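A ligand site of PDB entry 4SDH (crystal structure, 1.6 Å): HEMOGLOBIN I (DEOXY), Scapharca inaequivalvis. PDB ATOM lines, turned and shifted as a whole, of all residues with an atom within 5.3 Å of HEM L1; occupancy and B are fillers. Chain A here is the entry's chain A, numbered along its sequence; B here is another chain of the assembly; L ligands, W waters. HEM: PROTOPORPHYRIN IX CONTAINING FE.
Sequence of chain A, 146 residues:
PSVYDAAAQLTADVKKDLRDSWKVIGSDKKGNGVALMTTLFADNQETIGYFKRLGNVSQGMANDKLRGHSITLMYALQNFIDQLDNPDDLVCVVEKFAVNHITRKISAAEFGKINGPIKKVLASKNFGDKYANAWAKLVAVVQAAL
Water W1 bridges O2A of HEM L1 and O of Phe 97. Water W3 lies within hydrogen-bond range of NZ of Lys 96 of chain B (2.8 Å) and O1A of HEM L1 (2.8 Å). Water W4 lies within hydrogen-bond range of the backbone carbonyl oxygen of Tyr 50 (2.8 Å), the backbone NH of Arg 53 (3.1 Å) and an oxygen (O1D) of HEM L1 (3.5 Å).
Merely in contact with HEM L1: Tyr 50, Phe 97, Phe 111, Phe 51, Ile 106, His 69, Leu 73, Leu 54, Ile 114, Glu 110, Ala 76, Thr 72, Leu 77 and Thr 47. Hydrophobic or aromatic side chains within 4 Å of HEM L1: Tyr 50, Phe 51, Leu 54, His 69, Leu 73, Ala 76, Leu 77, Phe 97, His 101, Ile 106, Phe 111 and Ile 114. Of the 24 residues printed, 20 come within 4 Å of HEM L1. Along chain A the residues within 4 Å of HEM L1 span positions 47 to 114. The nearest printed residue that does not touch HEM L1 is Leu 40 (4.5 Å).
FE of HEM L1 is bound by NE2 of His 101, at 2.2 Å. O1A of HEM L2 is in hydrogen-bond range of ND2 of Asn 100 of chain A, 2.8 Å away. An oxygen (O2D) of HEM L1 is in salt-bridge range of the side-chain amino group (NZ) of Lys 96 of chain B, at 2.5 Å. O1A of HEM L1 sits at hydrogen-bond distance from ND2 of Asn 100 of chain B, at 3.0 Å. The guanidinium group of Arg 53 lies within salt-bridge range of an oxygen (O2D) of HEM L1 (2.7 Å). The side-chain amide nitrogen of Asn 100 of chain A lies close to an oxygen (O2A) of HEM L1. The side-chain amide nitrogen (ND2) of Asn 100 of chain B lies within hydrogen-bond range of an oxygen (O2A) of HEM L2, 3.3 Å away. The guanidinium group of Arg 104 is in salt-bridge range of an oxygen (O1A) of HEM L1, at 2.6 Å.
N of Ile 106 lies within hydrogen-bond range of O of His 101 (3.0 Å). O of Phe 97 sits at hydrogen-bond distance from ND1 of His 101 (3.1 Å). OE1 of Glu 110 lies within hydrogen-bond range of OH of Tyr 50, 2.6 Å away. The side-chain amide nitrogen (ND2) of Asn 100 of chain A sits close to the side-chain amide nitrogen (ND2) of Asn 100 of chain B. NZ of Lys 96 of chain B lies within hydrogen-bond range of ND1 of His 69 (2.9 Å).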
ATOM      1  N   LEU A  40     -26.414  -3.865   4.316  1.00  0.00           N
ATOM      2  CA  LEU A  40     -26.663  -2.635   5.109  1.00  0.00           C
ATOM      3  C   LEU A  40     -26.936  -1.462   4.173  1.00  0.00           C
ATOM      4  O   LEU A  40     -27.884  -0.709   4.401  1.00  0.00           O
ATOM      5  CB  LEU A  40     -25.413  -2.339   5.958  1.00  0.00           C
ATOM      6  CG  LEU A  40     -25.555  -1.076   6.775  1.00  0.00           C
ATOM      7  CD1 LEU A  40     -26.443  -1.286   7.998  1.00  0.00           C
ATOM      8  CD2 LEU A  40     -24.161  -0.661   7.253  1.00  0.00           C
ATOM      9  N   THR A  47     -27.337   5.177   5.747  1.00  0.00           N
ATOM     10  CA  THR A  47     -26.046   4.911   6.391  1.00  0.00           C
ATOM     11  C   THR A  47     -24.867   5.099   5.482  1.00  0.00           C
ATOM     12  O   THR A  47     -23.753   5.134   6.009  1.00  0.00           O
ATOM     13  CB  THR A  47     -25.967   3.479   7.080  1.00  0.00           C
ATOM     14  OG1 THR A  47     -26.108   2.526   5.967  1.00  0.00           O
ATOM     15  CG2 THR A  47     -26.959   3.284   8.245  1.00  0.00           C
ATOM     16  N   TYR A  50     -22.047   7.893   6.169  1.00  0.00           N
ATOM     17  CA  TYR A  50     -20.951   7.669   7.099  1.00  0.00           C
ATOM     18  C   TYR A  50     -19.722   7.090   6.386  1.00  0.00           C
ATOM     19  O   TYR A  50     -18.581   7.193   6.907  1.00  0.00           O
ATOM     20  CB  TYR A  50     -21.328   6.681   8.243  1.00  0.00           C
ATOM     21  CG  TYR A  50     -22.358   7.233   9.189  1.00  0.00           C
ATOM     22  CD1 TYR A  50     -22.079   8.293  10.065  1.00  0.00           C
ATOM     23  CD2 TYR A  50     -23.631   6.676   9.231  1.00  0.00           C
ATOM     24  CE1 TYR A  50     -23.071   8.745  10.963  1.00  0.00           C
ATOM     25  CE2 TYR A  50     -24.631   7.111  10.097  1.00  0.00           C
ATOM     26  CZ  TYR A  50     -24.342   8.177  10.964  1.00  0.00           C
ATOM     27  OH  TYR A  50     -25.347   8.604  11.808  1.00  0.00           O
ATOM     28  N   PHE A  51     -19.952   6.460   5.242  1.00  0.00           N
ATOM     29  CA  PHE A  51     -18.876   5.782   4.503  1.00  0.00           C
ATOM     30  C   PHE A  51     -18.365   6.506   3.271  1.00  0.00           C
ATOM     31  O   PHE A  51     -17.877   5.824   2.314  1.00  0.00           O
ATOM     32  CB  PHE A  51     -19.367   4.375   4.152  1.00  0.00           C
ATOM     33  CG  PHE A  51     -19.632   3.526   5.372  1.00  0.00           C
ATOM     34  CD1 PHE A  51     -18.594   2.744   5.900  1.00  0.00           C
ATOM     35  CD2 PHE A  51     -20.904   3.477   5.940  1.00  0.00           C
ATOM     36  CE1 PHE A  51     -18.806   1.935   7.010  1.00  0.00           C
ATOM     37  CE2 PHE A  51     -21.133   2.668   7.054  1.00  0.00           C
ATOM     38  CZ  PHE A  51     -20.100   1.876   7.604  1.00  0.00           C
ATOM     39  N   ARG A  53     -15.710   7.954   2.635  1.00  0.00           N
ATOM     40  CA  ARG A  53     -14.304   7.616   2.311  1.00  0.00           C
ATOM     41  C   ARG A  53     -14.211   6.416   1.380  1.00  0.00           C
ATOM     42  O   ARG A  53     -13.304   6.329   0.519  1.00  0.00           O
ATOM     43  CB  ARG A  53     -13.454   7.346   3.597  1.00  0.00           C
ATOM     44  CG  ARG A  53     -11.941   7.312   3.283  1.00  0.00           C
ATOM     45  CD  ARG A  53     -11.155   6.808   4.480  1.00  0.00           C
ATOM     46  NE  ARG A  53     -11.361   5.410   4.744  1.00  0.00           N
ATOM     47  CZ  ARG A  53     -10.710   4.417   4.100  1.00  0.00           C
ATOM     48  NH1 ARG A  53      -9.841   4.705   3.116  1.00  0.00           N
ATOM     49  NH2 ARG A  53     -10.885   3.153   4.475  1.00  0.00           N
ATOM     50  N   LEU A  54     -15.144   5.457   1.465  1.00  0.00           N
ATOM     51  CA  LEU A  54     -15.131   4.236   0.639  1.00  0.00           C
ATOM     52  C   LEU A  54     -15.415   4.418  -0.847  1.00  0.00           C
ATOM     53  O   LEU A  54     -15.156   3.488  -1.635  1.00  0.00           O
ATOM     54  CB  LEU A  54     -16.165   3.292   1.279  1.00  0.00           C
ATOM     55  CG  LEU A  54     -15.688   2.372   2.390  1.00  0.00           C
ATOM     56  CD1 LEU A  54     -14.661   3.008   3.315  1.00  0.00           C
ATOM     57  CD2 LEU A  54     -16.916   1.893   3.163  1.00  0.00           C
ATOM     58  N   HIS A  69     -12.357  -2.699   4.096  1.00  0.00           N
ATOM     59  CA  HIS A  69     -13.190  -2.431   5.307  1.00  0.00           C
ATOM     60  C   HIS A  69     -13.968  -3.674   5.751  1.00  0.00           C
ATOM     61  O   HIS A  69     -14.068  -4.050   6.929  1.00  0.00           O
ATOM     62  CB  HIS A  69     -14.179  -1.276   5.037  1.00  0.00           C
ATOM     63  CG  HIS A  69     -15.195  -1.132   6.127  1.00  0.00           C
ATOM     64  ND1 HIS A  69     -14.888  -0.558   7.328  1.00  0.00           N
ATOM     65  CD2 HIS A  69     -16.475  -1.598   6.176  1.00  0.00           C
ATOM     66  CE1 HIS A  69     -15.984  -0.665   8.083  1.00  0.00           C
ATOM     67  NE2 HIS A  69     -16.959  -1.250   7.432  1.00  0.00           N
ATOM     68  N   THR A  72     -11.858  -6.421   7.281  1.00  0.00           N
ATOM     69  CA  THR A  72     -11.476  -5.968   8.644  1.00  0.00           C
ATOM     70  C   THR A  72     -12.611  -6.043   9.641  1.00  0.00           C
ATOM     71  O   THR A  72     -12.374  -6.439  10.829  1.00  0.00           O
ATOM     72  CB  THR A  72     -10.883  -4.507   8.523  1.00  0.00           C
ATOM     73  OG1 THR A  72      -9.747  -4.633   7.622  1.00  0.00           O
ATOM     74  CG2 THR A  72     -10.461  -3.998   9.933  1.00  0.00           C
ATOM     75  N   LEU A  73     -13.807  -5.656   9.239  1.00  0.00           N
ATOM     76  CA  LEU A  73     -14.991  -5.767  10.136  1.00  0.00           C
ATOM     77  C   LEU A  73     -15.110  -7.212  10.681  1.00  0.00           C
ATOM     78  O   LEU A  73     -15.397  -7.419  11.894  1.00  0.00           O
ATOM     79  CB  LEU A  73     -16.194  -5.372   9.295  1.00  0.00           C
ATOM     80  CG  LEU A  73     -17.570  -5.546   9.975  1.00  0.00           C
ATOM     81  CD1 LEU A  73     -18.441  -4.429   9.440  1.00  0.00           C
ATOM     82  CD2 LEU A  73     -18.107  -6.958   9.650  1.00  0.00           C
ATOM     83  N   ALA A  76     -13.123  -7.998  13.756  1.00  0.00           N
ATOM     84  CA  ALA A  76     -13.630  -7.451  15.063  1.00  0.00           C
ATOM     85  C   ALA A  76     -14.644  -8.541  15.582  1.00  0.00           C
ATOM     86  O   ALA A  76     -14.701  -8.788  16.778  1.00  0.00           O
ATOM     87  CB  ALA A  76     -14.360  -6.127  14.890  1.00  0.00           C
ATOM     88  N   LEU A  77     -15.481  -9.042  14.666  1.00  0.00           N
ATOM     89  CA  LEU A  77     -16.401 -10.123  15.133  1.00  0.00           C
ATOM     90  C   LEU A  77     -15.601 -11.301  15.665  1.00  0.00           C
ATOM     91  O   LEU A  77     -15.976 -11.905  16.677  1.00  0.00           O
ATOM     92  CB  LEU A  77     -17.400 -10.454  14.051  1.00  0.00           C
ATOM     93  CG  LEU A  77     -18.417  -9.421  13.634  1.00  0.00           C
ATOM     94  CD1 LEU A  77     -19.410 -10.054  12.633  1.00  0.00           C
ATOM     95  CD2 LEU A  77     -19.199  -8.957  14.861  1.00  0.00           C
ATOM     96  N   PHE A  80     -14.521 -10.611  19.210  1.00  0.00           N
ATOM     97  CA  PHE A  80     -15.664 -10.764  20.124  1.00  0.00           C
ATOM     98  C   PHE A  80     -15.955 -12.261  20.389  1.00  0.00           C
ATOM     99  O   PHE A  80     -16.068 -12.615  21.567  1.00  0.00           O
ATOM    100  CB  PHE A  80     -16.916 -10.075  19.610  1.00  0.00           C
ATOM    101  CG  PHE A  80     -16.847  -8.607  19.383  1.00  0.00           C
ATOM    102  CD1 PHE A  80     -15.785  -7.860  19.950  1.00  0.00           C
ATOM    103  CD2 PHE A  80     -17.792  -7.943  18.601  1.00  0.00           C
ATOM    104  CE1 PHE A  80     -15.692  -6.482  19.756  1.00  0.00           C
ATOM    105  CE2 PHE A  80     -17.708  -6.546  18.399  1.00  0.00           C
ATOM    106  CZ  PHE A  80     -16.666  -5.835  18.978  1.00  0.00           C
ATOM    107  N   PHE A  97     -13.327  -1.160  20.961  1.00  0.00           N
ATOM    108  CA  PHE A  97     -13.988  -1.073  19.645  1.00  0.00           C
ATOM    109  C   PHE A  97     -14.898   0.143  19.547  1.00  0.00           C
ATOM    110  O   PHE A  97     -15.017   0.793  18.497  1.00  0.00           O
ATOM    111  CB  PHE A  97     -14.859  -2.363  19.474  1.00  0.00           C
ATOM    112  CG  PHE A  97     -15.763  -2.327  18.292  1.00  0.00           C
ATOM    113  CD1 PHE A  97     -17.064  -1.859  18.370  1.00  0.00           C
ATOM    114  CD2 PHE A  97     -15.297  -2.911  17.078  1.00  0.00           C
ATOM    115  CE1 PHE A  97     -17.938  -1.898  17.276  1.00  0.00           C
ATOM    116  CE2 PHE A  97     -16.159  -2.909  15.967  1.00  0.00           C
ATOM    117  CZ  PHE A  97     -17.438  -2.395  16.065  1.00  0.00           C
ATOM    118  N   ASN A 100     -13.713   4.474  18.387  1.00  0.00           N
ATOM    119  CA  ASN A 100     -13.816   5.061  17.049  1.00  0.00           C
ATOM    120  C   ASN A 100     -15.241   5.305  16.623  1.00  0.00           C
ATOM    121  O   ASN A 100     -15.491   6.282  15.891  1.00  0.00           O
ATOM    122  CB  ASN A 100     -13.003   4.236  16.040  1.00  0.00           C
ATOM    123  CG  ASN A 100     -11.495   4.368  16.326  1.00  0.00           C
ATOM    124  OD1 ASN A 100     -11.042   5.234  17.090  1.00  0.00           O
ATOM    125  ND2 ASN A 100     -10.740   3.460  15.726  1.00  0.00           N
ATOM    126  N   HIS A 101     -16.151   4.379  17.009  1.00  0.00           N
ATOM    127  CA  HIS A 101     -17.568   4.518  16.602  1.00  0.00           C
ATOM    128  C   HIS A 101     -18.190   5.697  17.310  1.00  0.00           C
ATOM    129  O   HIS A 101     -18.929   6.454  16.689  1.00  0.00           O
ATOM    130  CB  HIS A 101     -18.369   3.203  16.788  1.00  0.00           C
ATOM    131  CG  HIS A 101     -17.858   2.161  15.833  1.00  0.00           C
ATOM    132  ND1 HIS A 101     -16.737   1.394  16.013  1.00  0.00           N
ATOM    133  CD2 HIS A 101     -18.336   1.809  14.593  1.00  0.00           C
ATOM    134  CE1 HIS A 101     -16.574   0.565  14.981  1.00  0.00           C
ATOM    135  NE2 HIS A 101     -17.500   0.851  14.072  1.00  0.00           N
ATOM    136  N   ARG A 104     -17.155   8.864  15.621  1.00  0.00           N
ATOM    137  CA  ARG A 104     -17.885   9.047  14.374  1.00  0.00           C
ATOM    138  C   ARG A 104     -19.354   9.384  14.595  1.00  0.00           C
ATOM    139  O   ARG A 104     -20.115   9.594  13.594  1.00  0.00           O
ATOM    140  CB  ARG A 104     -17.858   7.831  13.486  1.00  0.00           C
ATOM    141  CG  ARG A 104     -16.537   7.464  12.901  1.00  0.00           C
ATOM    142  CD  ARG A 104     -16.701   5.978  12.415  1.00  0.00           C
ATOM    143  NE  ARG A 104     -15.346   5.637  12.149  1.00  0.00           N
ATOM    144  CZ  ARG A 104     -14.643   4.570  12.568  1.00  0.00           C
ATOM    145  NH1 ARG A 104     -15.200   3.518  13.221  1.00  0.00           N
ATOM    146  NH2 ARG A 104     -13.326   4.805  12.382  1.00  0.00           N
ATOM    147  N   ILE A 106     -21.660   7.431  15.893  1.00  0.00           N
ATOM    148  CA  ILE A 106     -22.597   6.329  15.557  1.00  0.00           C
ATOM    149  C   ILE A 106     -23.321   6.061  16.873  1.00  0.00           C
ATOM    150  O   ILE A 106     -22.599   5.636  17.813  1.00  0.00           O
ATOM    151  CB  ILE A 106     -21.819   5.081  15.054  1.00  0.00           C
ATOM    152  CG1 ILE A 106     -20.903   5.454  13.867  1.00  0.00           C
ATOM    153  CG2 ILE A 106     -22.823   3.916  14.729  1.00  0.00           C
ATOM    154  CD1 ILE A 106     -21.650   5.883  12.605  1.00  0.00           C
ATOM    155  N   GLU A 110     -28.244   3.643  15.582  1.00  0.00           N
ATOM    156  CA  GLU A 110     -27.618   3.551  14.263  1.00  0.00           C
ATOM    157  C   GLU A 110     -26.890   2.215  14.127  1.00  0.00           C
ATOM    158  O   GLU A 110     -26.992   1.539  13.081  1.00  0.00           O
ATOM    159  CB  GLU A 110     -26.556   4.631  14.088  1.00  0.00           C
ATOM    160  CG  GLU A 110     -26.283   5.017  12.634  1.00  0.00           C
ATOM    161  CD  GLU A 110     -27.267   6.113  12.193  1.00  0.00           C
ATOM    162  OE1 GLU A 110     -27.292   7.190  12.794  1.00  0.00           O
ATOM    163  OE2 GLU A 110     -27.952   5.726  11.232  1.00  0.00           O
ATOM    164  N   PHE A 111     -26.101   1.875  15.128  1.00  0.00           N
ATOM    165  CA  PHE A 111     -25.333   0.617  15.134  1.00  0.00           C
ATOM    166  C   PHE A 111     -26.260  -0.622  15.005  1.00  0.00           C
ATOM    167  O   PHE A 111     -25.904  -1.613  14.350  1.00  0.00           O
ATOM    168  CB  PHE A 111     -24.488   0.511  16.398  1.00  0.00           C
ATOM    169  CG  PHE A 111     -23.390  -0.513  16.301  1.00  0.00           C
ATOM    170  CD1 PHE A 111     -22.136  -0.159  15.792  1.00  0.00           C
ATOM    171  CD2 PHE A 111     -23.606  -1.822  16.715  1.00  0.00           C
ATOM    172  CE1 PHE A 111     -21.131  -1.128  15.688  1.00  0.00           C
ATOM    173  CE2 PHE A 111     -22.595  -2.799  16.682  1.00  0.00           C
ATOM    174  CZ  PHE A 111     -21.366  -2.425  16.102  1.00  0.00           C
ATOM    175  N   ILE A 114     -27.273  -2.935  11.937  1.00  0.00           N
ATOM    176  CA  ILE A 114     -26.562  -4.085  11.414  1.00  0.00           C
ATOM    177  C   ILE A 114     -27.334  -5.400  11.668  1.00  0.00           C
ATOM    178  O   ILE A 114     -27.045  -6.391  10.985  1.00  0.00           O
ATOM    179  CB  ILE A 114     -25.155  -4.191  12.108  1.00  0.00           C
ATOM    180  CG1 ILE A 114     -24.252  -4.982  11.105  1.00  0.00           C
ATOM    181  CG2 ILE A 114     -25.223  -4.673  13.560  1.00  0.00           C
ATOM    182  CD1 ILE A 114     -23.998  -4.086   9.823  1.00  0.00           C
ATOM    183  N   ILE A 118     -27.258  -8.827   9.512  1.00  0.00           N
ATOM    184  CA  ILE A 118     -26.762 -10.108  10.057  1.00  0.00           C
ATOM    185  C   ILE A 118     -27.787 -11.238   9.859  1.00  0.00           C
ATOM    186  O   ILE A 118     -27.458 -12.380   9.499  1.00  0.00           O
ATOM    187  CB  ILE A 118     -26.294  -9.978  11.527  1.00  0.00           C
ATOM    188  CG1 ILE A 118     -25.022  -9.054  11.546  1.00  0.00           C
ATOM    189  CG2 ILE A 118     -26.019 -11.305  12.248  1.00  0.00           C
ATOM    190  CD1 ILE A 118     -24.648  -8.622  12.989  1.00  0.00           C
ATOM    191  N   VAL A 139     -24.616  -7.900  19.652  1.00  0.00           N
ATOM    192  CA  VAL A 139     -24.668  -6.519  19.131  1.00  0.00           C
ATOM    193  C   VAL A 139     -25.154  -5.574  20.244  1.00  0.00           C
ATOM    194  O   VAL A 139     -24.633  -4.451  20.359  1.00  0.00           O
ATOM    195  CB  VAL A 139     -25.481  -6.458  17.803  1.00  0.00           C
ATOM    196  CG1 VAL A 139     -25.829  -5.040  17.362  1.00  0.00           C
ATOM    197  CG2 VAL A 139     -24.748  -7.185  16.680  1.00  0.00           C
ATOM    198  N   LYS B  96      -6.415   0.005   4.589  1.00  0.00           N
ATOM    199  CA  LYS B  96      -7.565   0.251   5.497  1.00  0.00           C
ATOM    200  C   LYS B  96      -7.003   0.476   6.904  1.00  0.00           C
ATOM    201  O   LYS B  96      -7.411   1.431   7.558  1.00  0.00           O
ATOM    202  CB  LYS B  96      -8.544  -0.895   5.500  1.00  0.00           C
ATOM    203  CG  LYS B  96      -9.575  -1.012   6.640  1.00  0.00           C
ATOM    204  CD  LYS B  96     -10.556   0.139   6.674  1.00  0.00           C
ATOM    205  CE  LYS B  96     -11.547  -0.093   7.838  1.00  0.00           C
ATOM    206  NZ  LYS B  96     -12.497   1.005   8.054  1.00  0.00           N
ATOM    207  N   ASN B 100      -6.394   5.097  10.112  1.00  0.00           N
ATOM    208  CA  ASN B 100      -6.397   5.764  11.462  1.00  0.00           C
ATOM    209  C   ASN B 100      -5.017   6.127  11.970  1.00  0.00           C
ATOM    210  O   ASN B 100      -4.893   7.039  12.831  1.00  0.00           O
ATOM    211  CB  ASN B 100      -7.095   4.922  12.514  1.00  0.00           C
ATOM    212  CG  ASN B 100      -8.592   4.805  12.273  1.00  0.00           C
ATOM    213  OD1 ASN B 100      -9.224   5.623  11.570  1.00  0.00           O
ATOM    214  ND2 ASN B 100      -9.170   3.732  12.889  1.00  0.00           N
HETATM  215  CHA HEM L   1     -14.834   1.228  10.914  1.00  0.00           C
HETATM  216  CHB HEM L   1     -16.305  -2.971  12.712  1.00  0.00           C
HETATM  217  CHC HEM L   1     -20.907  -1.523  12.281  1.00  0.00           C
HETATM  218  CHD HEM L   1     -19.392   2.816  10.833  1.00  0.00           C
HETATM  219  C1A HEM L   1     -14.785  -0.020  11.511  1.00  0.00           C
HETATM  220  C2A HEM L   1     -13.592  -0.780  11.786  1.00  0.00           C
HETATM  221  C3A HEM L   1     -13.998  -1.994  12.264  1.00  0.00           C
HETATM  222  C4A HEM L   1     -15.453  -1.965  12.270  1.00  0.00           C
HETATM  223  CMA HEM L   1     -13.107  -3.137  12.758  1.00  0.00           C
HETATM  224  CAA HEM L   1     -12.150  -0.313  11.581  1.00  0.00           C
HETATM  225  CBA HEM L   1     -11.516   0.333  12.854  1.00  0.00           C
HETATM  226  CGA HEM L   1     -12.204   1.618  13.252  1.00  0.00           C
HETATM  227  O1A HEM L   1     -11.883   2.595  12.510  1.00  0.00           O
HETATM  228  O2A HEM L   1     -13.007   1.701  14.211  1.00  0.00           O
HETATM  229  C1B HEM L   1     -17.688  -2.934  12.745  1.00  0.00           C
HETATM  230  C2B HEM L   1     -18.533  -4.054  13.174  1.00  0.00           C
HETATM  231  C3B HEM L   1     -19.791  -3.646  13.063  1.00  0.00           C
HETATM  232  C4B HEM L   1     -19.770  -2.291  12.523  1.00  0.00           C
HETATM  233  CMB HEM L   1     -17.954  -5.405  13.681  1.00  0.00           C
HETATM  234  CAB HEM L   1     -21.068  -4.407  13.389  1.00  0.00           C
HETATM  235  CBB HEM L   1     -21.221  -5.691  13.223  1.00  0.00           C
HETATM  236  C1C HEM L   1     -20.885  -0.232  11.824  1.00  0.00           C
HETATM  237  C2C HEM L   1     -22.092   0.562  11.546  1.00  0.00           C
HETATM  238  C3C HEM L   1     -21.660   1.742  11.165  1.00  0.00           C
HETATM  239  C4C HEM L   1     -20.201   1.747  11.197  1.00  0.00           C
HETATM  240  CMC HEM L   1     -23.516   0.000  11.650  1.00  0.00           C
HETATM  241  CAC HEM L   1     -22.390   2.980  10.635  1.00  0.00           C
HETATM  242  CBC HEM L   1     -23.706   3.085  10.545  1.00  0.00           C
HETATM  243  C1D HEM L   1     -18.043   2.712  10.592  1.00  0.00           C
HETATM  244  C2D HEM L   1     -17.259   3.633   9.766  1.00  0.00           C
HETATM  245  C3D HEM L   1     -16.017   3.202   9.787  1.00  0.00           C
HETATM  246  C4D HEM L   1     -15.961   2.004  10.596  1.00  0.00           C
HETATM  247  CMD HEM L   1     -17.895   4.861   9.022  1.00  0.00           C
HETATM  248  CAD HEM L   1     -14.815   3.799   9.017  1.00  0.00           C
HETATM  249  CBD HEM L   1     -14.877   3.319   7.525  1.00  0.00           C
HETATM  250  CGD HEM L   1     -13.644   3.758   6.763  1.00  0.00           C
HETATM  251  O1D HEM L   1     -13.624   4.981   6.524  1.00  0.00           O
HETATM  252  O2D HEM L   1     -12.766   2.947   6.466  1.00  0.00           O
HETATM  253  NA  HEM L   1     -15.927  -0.753  11.830  1.00  0.00           N
HETATM  254  NB  HEM L   1     -18.479  -1.877  12.347  1.00  0.00           N
HETATM  255  NC  HEM L   1     -19.725   0.507  11.667  1.00  0.00           N
HETATM  256  ND  HEM L   1     -17.211   1.710  11.080  1.00  0.00           N
HETATM  257 FE   HEM L   1     -17.805   0.035  12.067  1.00  0.00          FE
HETATM  258  CHA HEM L   2      -4.924   1.687  17.550  1.00  0.00           C
HETATM  259  CHB HEM L   2      -2.889  -2.181  15.514  1.00  0.00           C
HETATM  260  CHC HEM L   2       1.451  -0.094  16.018  1.00  0.00           C
HETATM  261  CHD HEM L   2      -0.621   3.922  17.767  1.00  0.00           C
HETATM  262  C1A HEM L   2      -4.763   0.479  16.860  1.00  0.00           C
HETATM  263  C2A HEM L   2      -5.835  -0.427  16.508  1.00  0.00           C
HETATM  264  C3A HEM L   2      -5.250  -1.498  15.923  1.00  0.00           C
HETATM  265  C4A HEM L   2      -3.833  -1.281  15.983  1.00  0.00           C
HETATM  266  CMA HEM L   2      -5.875  -2.764  15.325  1.00  0.00           C
HETATM  267  CAA HEM L   2      -7.344  -0.206  16.653  1.00  0.00           C
HETATM  268  CBA HEM L   2      -8.024   0.371  15.414  1.00  0.00           C
HETATM  269  CGA HEM L   2      -7.569   1.788  15.147  1.00  0.00           C
HETATM  270  O1A HEM L   2      -8.013   2.691  15.911  1.00  0.00           O
HETATM  271  O2A HEM L   2      -6.743   2.043  14.266  1.00  0.00           O
HETATM  272  C1B HEM L   2      -1.527  -1.972  15.542  1.00  0.00           C
HETATM  273  C2B HEM L   2      -0.532  -2.946  15.057  1.00  0.00           C
HETATM  274  C3B HEM L   2       0.654  -2.370  15.185  1.00  0.00           C
HETATM  275  C4B HEM L   2       0.431  -1.028  15.727  1.00  0.00           C
HETATM  276  CMB HEM L   2      -0.845  -4.361  14.492  1.00  0.00           C
HETATM  277  CAB HEM L   2       2.055  -2.901  14.864  1.00  0.00           C
HETATM  278  CBB HEM L   2       2.444  -4.138  14.587  1.00  0.00           C
HETATM  279  C1C HEM L   2       1.257   1.180  16.544  1.00  0.00           C
HETATM  280  C2C HEM L   2       2.365   2.098  16.875  1.00  0.00           C
HETATM  281  C3C HEM L   2       1.765   3.219  17.385  1.00  0.00           C
HETATM  282  C4C HEM L   2       0.339   3.021  17.316  1.00  0.00           C
HETATM  283  CMC HEM L   2       3.828   1.712  16.742  1.00  0.00           C
HETATM  284  CAC HEM L   2       2.387   4.514  17.908  1.00  0.00           C
HETATM  285  CBC HEM L   2       3.659   4.691  18.207  1.00  0.00           C
HETATM  286  C1D HEM L   2      -1.944   3.617  17.924  1.00  0.00           C
HETATM  287  C2D HEM L   2      -2.851   4.367  18.792  1.00  0.00           C
HETATM  288  C3D HEM L   2      -4.048   3.773  18.708  1.00  0.00           C
HETATM  289  C4D HEM L   2      -3.892   2.600  17.840  1.00  0.00           C
HETATM  290  CMD HEM L   2      -2.451   5.637  19.608  1.00  0.00           C
HETATM  291  CAD HEM L   2      -5.353   4.121  19.471  1.00  0.00           C
HETATM  292  CBD HEM L   2      -5.180   3.676  20.935  1.00  0.00           C
HETATM  293  CGD HEM L   2      -6.397   3.898  21.789  1.00  0.00           C
HETATM  294  O1D HEM L   2      -6.585   5.059  22.258  1.00  0.00           O
HETATM  295  O2D HEM L   2      -7.189   2.956  22.005  1.00  0.00           O
HETATM  296  NA  HEM L   2      -3.543  -0.044  16.507  1.00  0.00           N
HETATM  297  NB  HEM L   2      -0.884  -0.799  15.927  1.00  0.00           N
HETATM  298  NC  HEM L   2       0.033   1.785  16.752  1.00  0.00           N
HETATM  299  ND  HEM L   2      -2.607   2.487  17.419  1.00  0.00           N
HETATM  300 FE   HEM L   2      -1.784   1.007  16.305  1.00  0.00          FE
HETATM  301  O   HOH W   1     -13.076   0.156  16.203  1.00  0.00           O
HETATM  302  O   HOH W   2     -12.746   7.204   7.915  1.00  0.00           O
HETATM  303  O   HOH W   3     -10.944   2.463   9.863  1.00  0.00           O
HETATM  304  O   HOH W   4     -16.121   7.233   5.586  1.00  0.00           O
HETATM  305  O   HOH W   5     -19.369  -1.267   9.180  1.00  0.00           O
